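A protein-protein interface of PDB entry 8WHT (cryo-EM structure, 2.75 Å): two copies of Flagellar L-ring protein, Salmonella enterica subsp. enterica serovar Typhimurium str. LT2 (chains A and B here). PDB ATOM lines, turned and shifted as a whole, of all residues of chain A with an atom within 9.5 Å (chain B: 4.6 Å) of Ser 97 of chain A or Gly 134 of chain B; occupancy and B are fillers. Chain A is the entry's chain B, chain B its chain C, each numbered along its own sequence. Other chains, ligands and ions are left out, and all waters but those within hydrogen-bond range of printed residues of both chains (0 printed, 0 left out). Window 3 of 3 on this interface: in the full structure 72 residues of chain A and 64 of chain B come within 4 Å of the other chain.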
ATOM      1  N   ALA A  94      20.658 -24.397 -14.608  1.00  0.00           N
ATOM      2  CA  ALA A  94      19.233 -24.593 -14.399  1.00  0.00           C
ATOM      3  C   ALA A  94      18.495 -24.145 -15.650  1.00  0.00           C
ATOM      4  O   ALA A  94      18.969 -23.266 -16.375  1.00  0.00           O
ATOM      5  CB  ALA A  94      18.729 -23.822 -13.175  1.00  0.00           C
ATOM      6  N   ASN A  95      17.350 -24.766 -15.913  1.00  0.00           N
ATOM      7  CA  ASN A  95      16.557 -24.408 -17.077  1.00  0.00           C
ATOM      8  C   ASN A  95      15.094 -24.708 -16.801  1.00  0.00           C
ATOM      9  O   ASN A  95      14.754 -25.535 -15.952  1.00  0.00           O
ATOM     10  CB  ASN A  95      17.029 -25.149 -18.334  1.00  0.00           C
ATOM     11  CG  ASN A  95      16.981 -26.655 -18.178  1.00  0.00           C
ATOM     12  OD1 ASN A  95      17.959 -27.280 -17.770  1.00  0.00           O
ATOM     13  ND2 ASN A  95      15.843 -27.249 -18.513  1.00  0.00           N
ATOM     14  N   ALA A  96      14.230 -24.017 -17.538  1.00  0.00           N
ATOM     15  CA  ALA A  96      12.796 -24.244 -17.460  1.00  0.00           C
ATOM     16  C   ALA A  96      12.164 -23.829 -18.779  1.00  0.00           C
ATOM     17  O   ALA A  96      12.547 -22.822 -19.377  1.00  0.00           O
ATOM     18  CB  ALA A  96      12.157 -23.479 -16.296  1.00  0.00           C
ATOM     19  N   SER A  97      11.190 -24.615 -19.229  1.00  0.00           N
ATOM     20  CA  SER A  97      10.550 -24.345 -20.506  1.00  0.00           C
ATOM     21  C   SER A  97       9.064 -24.651 -20.398  1.00  0.00           C
ATOM     22  O   SER A  97       8.636 -25.489 -19.601  1.00  0.00           O
ATOM     23  CB  SER A  97      11.186 -25.161 -21.637  1.00  0.00           C
ATOM     24  OG  SER A  97      10.798 -24.667 -22.905  1.00  0.00           O
ATOM     25  N   ARG A  98       8.282 -23.952 -21.217  1.00  0.00           N
ATOM     26  CA  ARG A  98       6.832 -24.122 -21.229  1.00  0.00           C
ATOM     27  C   ARG A  98       6.321 -23.707 -22.597  1.00  0.00           C
ATOM     28  O   ARG A  98       6.567 -22.579 -23.030  1.00  0.00           O
ATOM     29  CB  ARG A  98       6.177 -23.289 -20.132  1.00  0.00           C
ATOM     30  CG  ARG A  98       4.695 -23.554 -19.948  1.00  0.00           C
ATOM     31  CD  ARG A  98       4.215 -23.042 -18.603  1.00  0.00           C
ATOM     32  NE  ARG A  98       3.556 -21.748 -18.715  1.00  0.00           N
ATOM     33  CZ  ARG A  98       2.829 -21.195 -17.755  1.00  0.00           C
ATOM     34  NH1 ARG A  98       2.659 -21.793 -16.587  1.00  0.00           N
ATOM     35  NH2 ARG A  98       2.257 -20.014 -17.972  1.00  0.00           N
ATOM     36  N   ASP A  99       5.617 -24.609 -23.276  1.00  0.00           N
ATOM     37  CA  ASP A  99       5.037 -24.331 -24.582  1.00  0.00           C
ATOM     38  C   ASP A  99       3.575 -24.747 -24.567  1.00  0.00           C
ATOM     39  O   ASP A  99       3.251 -25.866 -24.157  1.00  0.00           O
ATOM     40  CB  ASP A  99       5.783 -25.072 -25.696  1.00  0.00           C
ATOM     41  CG  ASP A  99       7.004 -24.317 -26.184  1.00  0.00           C
ATOM     42  OD1 ASP A  99       7.642 -23.619 -25.370  1.00  0.00           O
ATOM     43  OD2 ASP A  99       7.322 -24.418 -27.386  1.00  0.00           O
ATOM     44  N   GLY A 100       2.697 -23.854 -25.013  1.00  0.00           N
ATOM     45  CA  GLY A 100       1.283 -24.161 -25.055  1.00  0.00           C
ATOM     46  C   GLY A 100       0.600 -23.659 -26.307  1.00  0.00           C
ATOM     47  O   GLY A 100       0.715 -22.482 -26.655  1.00  0.00           O
ATOM     48  N   GLY A 128       1.611 -19.743 -26.697  1.00  0.00           N
ATOM     49  CA  GLY A 128       2.432 -19.115 -25.681  1.00  0.00           C
ATOM     50  C   GLY A 128       3.677 -19.929 -25.403  1.00  0.00           C
ATOM     51  O   GLY A 128       3.686 -21.158 -25.526  1.00  0.00           O
ATOM     52  N   GLY A 129       4.733 -19.221 -25.016  1.00  0.00           N
ATOM     53  CA  GLY A 129       6.003 -19.861 -24.735  1.00  0.00           C
ATOM     54  C   GLY A 129       6.761 -19.115 -23.663  1.00  0.00           C
ATOM     55  O   GLY A 129       6.650 -17.893 -23.535  1.00  0.00           O
ATOM     56  N   ASN A 130       7.538 -19.865 -22.890  1.00  0.00           N
ATOM     57  CA  ASN A 130       8.375 -19.312 -21.834  1.00  0.00           C
ATOM     58  C   ASN A 130       9.633 -20.162 -21.748  1.00  0.00           C
ATOM     59  O   ASN A 130       9.541 -21.389 -21.672  1.00  0.00           O
ATOM     60  CB  ASN A 130       7.638 -19.299 -20.491  1.00  0.00           C
ATOM     61  CG  ASN A 130       7.997 -18.098 -19.639  1.00  0.00           C
ATOM     62  OD1 ASN A 130       9.099 -18.012 -19.098  1.00  0.00           O
ATOM     63  ND2 ASN A 130       7.065 -17.164 -19.515  1.00  0.00           N
ATOM     64  N   SER A 131      10.798 -19.519 -21.769  1.00  0.00           N
ATOM     65  CA  SER A 131      12.062 -20.240 -21.763  1.00  0.00           C
ATOM     66  C   SER A 131      13.049 -19.546 -20.838  1.00  0.00           C
ATOM     67  O   SER A 131      13.091 -18.317 -20.756  1.00  0.00           O
ATOM     68  CB  SER A 131      12.650 -20.346 -23.176  1.00  0.00           C
ATOM     69  OG  SER A 131      13.492 -21.477 -23.295  1.00  0.00           O
ATOM     70  N   PHE A 132      13.845 -20.352 -20.137  1.00  0.00           N
ATOM     71  CA  PHE A 132      14.885 -19.835 -19.263  1.00  0.00           C
ATOM     72  C   PHE A 132      16.021 -20.844 -19.202  1.00  0.00           C
ATOM     73  O   PHE A 132      15.781 -22.040 -19.019  1.00  0.00           O
ATOM     74  CB  PHE A 132      14.357 -19.556 -17.853  1.00  0.00           C
ATOM     75  CG  PHE A 132      15.429 -19.174 -16.876  1.00  0.00           C
ATOM     76  CD1 PHE A 132      15.978 -17.905 -16.892  1.00  0.00           C
ATOM     77  CD2 PHE A 132      15.900 -20.090 -15.951  1.00  0.00           C
ATOM     78  CE1 PHE A 132      16.970 -17.556 -16.004  1.00  0.00           C
ATOM     79  CE2 PHE A 132      16.893 -19.745 -15.061  1.00  0.00           C
ATOM     80  CZ  PHE A 132      17.427 -18.477 -15.086  1.00  0.00           C
ATOM     81  N   ASN A 133      17.249 -20.348 -19.340  1.00  0.00           N
ATOM     82  CA  ASN A 133      18.444 -21.187 -19.273  1.00  0.00           C
ATOM     83  C   ASN A 133      19.555 -20.372 -18.628  1.00  0.00           C
ATOM     84  O   ASN A 133      20.076 -19.440 -19.248  1.00  0.00           O
ATOM     85  CB  ASN A 133      18.858 -21.666 -20.661  1.00  0.00           C
ATOM     86  CG  ASN A 133      18.201 -22.974 -21.048  1.00  0.00           C
ATOM     87  OD1 ASN A 133      18.770 -24.047 -20.856  1.00  0.00           O
ATOM     88  ND2 ASN A 133      16.996 -22.890 -21.598  1.00  0.00           N
ATOM     89  N   SER B  93       9.567 -33.290 -16.391  1.00  0.00           N
ATOM     90  CA  SER B  93       8.805 -32.774 -17.517  1.00  0.00           C
ATOM     91  C   SER B  93       7.376 -33.288 -17.423  1.00  0.00           C
ATOM     92  O   SER B  93       7.087 -34.257 -16.717  1.00  0.00           O
ATOM     93  CB  SER B  93       9.433 -33.176 -18.857  1.00  0.00           C
ATOM     94  OG  SER B  93       9.698 -34.566 -18.901  1.00  0.00           O
ATOM     95  N   ALA B  94       6.485 -32.616 -18.146  1.00  0.00           N
ATOM     96  CA  ALA B  94       5.085 -33.002 -18.228  1.00  0.00           C
ATOM     97  C   ALA B  94       4.534 -32.538 -19.566  1.00  0.00           C
ATOM     98  O   ALA B  94       5.007 -31.547 -20.129  1.00  0.00           O
ATOM     99  CB  ALA B  94       4.267 -32.409 -17.076  1.00  0.00           C
ATOM    100  N   PHE B 132       0.304 -28.957 -24.609  1.00  0.00           N
ATOM    101  CA  PHE B 132       1.088 -28.396 -23.520  1.00  0.00           C
ATOM    102  C   PHE B 132       2.321 -29.262 -23.307  1.00  0.00           C
ATOM    103  O   PHE B 132       2.216 -30.489 -23.251  1.00  0.00           O
ATOM    104  CB  PHE B 132       0.279 -28.309 -22.223  1.00  0.00           C
ATOM    105  CG  PHE B 132       1.094 -27.888 -21.035  1.00  0.00           C
ATOM    106  CD1 PHE B 132       1.459 -26.566 -20.866  1.00  0.00           C
ATOM    107  CD2 PHE B 132       1.509 -28.818 -20.099  1.00  0.00           C
ATOM    108  CE1 PHE B 132       2.216 -26.178 -19.784  1.00  0.00           C
ATOM    109  CE2 PHE B 132       2.268 -28.435 -19.014  1.00  0.00           C
ATOM    110  CZ  PHE B 132       2.621 -27.114 -18.856  1.00  0.00           C
ATOM    111  N   ASN B 133       3.474 -28.610 -23.176  1.00  0.00           N
ATOM    112  CA  ASN B 133       4.740 -29.299 -22.934  1.00  0.00           C
ATOM    113  C   ASN B 133       5.594 -28.416 -22.037  1.00  0.00           C
ATOM    114  O   ASN B 133       6.087 -27.377 -22.485  1.00  0.00           O
ATOM    115  CB  ASN B 133       5.461 -29.601 -24.245  1.00  0.00           C
ATOM    116  CG  ASN B 133       5.069 -30.939 -24.833  1.00  0.00           C
ATOM    117  OD1 ASN B 133       5.735 -31.948 -24.605  1.00  0.00           O
ATOM    118  ND2 ASN B 133       3.983 -30.954 -25.598  1.00  0.00           N
ATOM    119  N   GLY B 134       5.772 -28.821 -20.785  1.00  0.00           N
ATOM    120  CA  GLY B 134       6.652 -28.126 -19.868  1.00  0.00           C
ATOM    121  C   GLY B 134       7.767 -29.042 -19.407  1.00  0.00           C
ATOM    122  O   GLY B 134       7.604 -30.260 -19.355  1.00  0.00           O
ATOM    123  N   LYS B 135       8.913 -28.449 -19.089  1.00  0.00           N
ATOM    124  CA  LYS B 135      10.043 -29.219 -18.592  1.00  0.00           C
ATOM    125  C   LYS B 135      10.947 -28.305 -17.783  1.00  0.00           C
ATOM    126  O   LYS B 135      10.864 -27.079 -17.882  1.00  0.00           O
ATOM    127  CB  LYS B 135      10.829 -29.876 -19.732  1.00  0.00           C
ATOM    128  CG  LYS B 135      11.495 -28.894 -20.676  1.00  0.00           C
ATOM    129  CD  LYS B 135      11.860 -29.562 -21.989  1.00  0.00           C
ATOM    130  CE  LYS B 135      13.273 -29.210 -22.411  1.00  0.00           C
ATOM    131  NZ  LYS B 135      13.701 -29.987 -23.603  1.00  0.00           N
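The backbone NH of Ser 97 of chain A sits at hydrogen-bond distance from the backbone carbonyl oxygen of Lys 135 of chain B (2.8 Å). The backbone carbonyl oxygen (O) of Asn 133 of chain B sits at hydrogen-bond distance from the backbone NH (N) of Asp 99 of chain A (2.9 Å).
O of Ala 96 of chain A lies within hydrogen-bond range of N of Phe 132 of chain A, at 2.9 Å. N of Asn 130 of chain A sits at hydrogen-bond distance from O of Arg 98 of chain A. O of Gly 134 of chain B lies within hydrogen-bond range of N of Ala 94 of chain B (2.9 Å).
Of the 13 printed residues of chain A, 4 touch a printed residue of chain B. Hydrophobic or aromatic side chains of chain B that line the printed part of chain A: Phe 132. Along chain B the printed residues that touch a printed residue of chain A span positions 132 to 135. Among the printed residues, 7 pairs touch across the chains. Among the printed residues, no Asp or Glu carboxylate lies within 4 Å of a Lys or Arg side-chain nitrogen of the other chain.
3 positions are printed for both chains. Of the 7 pairs that touch across the chains among the printed residues, none has its exchanged pair printed and touching as well.
Printed residues of chain B within 4 Å of Ala 96 of chain A: Lys 135 (3.5 Å). Ser 97 of chain A touches just these residues of chain B: Gly 134 and Lys 135. Gly 128 of chain A touches none of the printed residues of chain B. Gly 129 of chain A touches none of the printed residues of chain B. No residue of chain A comes within 4 Å of Ala 94 of chain B. Of the printed residues of chain A, Asn 133 of chain B touches Arg 98 and Asp 99. Gly 134 of chain B touches just one residue of chain A: Ser 97 (3.3 Å). Of the printed residues of chain A, Lys 135 of chain B touches Ala 96 and Ser 97. The nearest printed residue of chain B that does not touch Asp 99 of chain A is Gly 134 of chain B (4.9 Å).
Among the printed residues, pairs that only touch across the chains: Ser 97 of chain A with Gly 134 of chain B, Asp 99 of chain A with Phe 132 of chain B, Ala 96 of chain A with Lys 135 of chain B, Arg 98 of chain A with Asn 133 of chain B and Arg 98 of chain A with Phe 132 of chain B.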
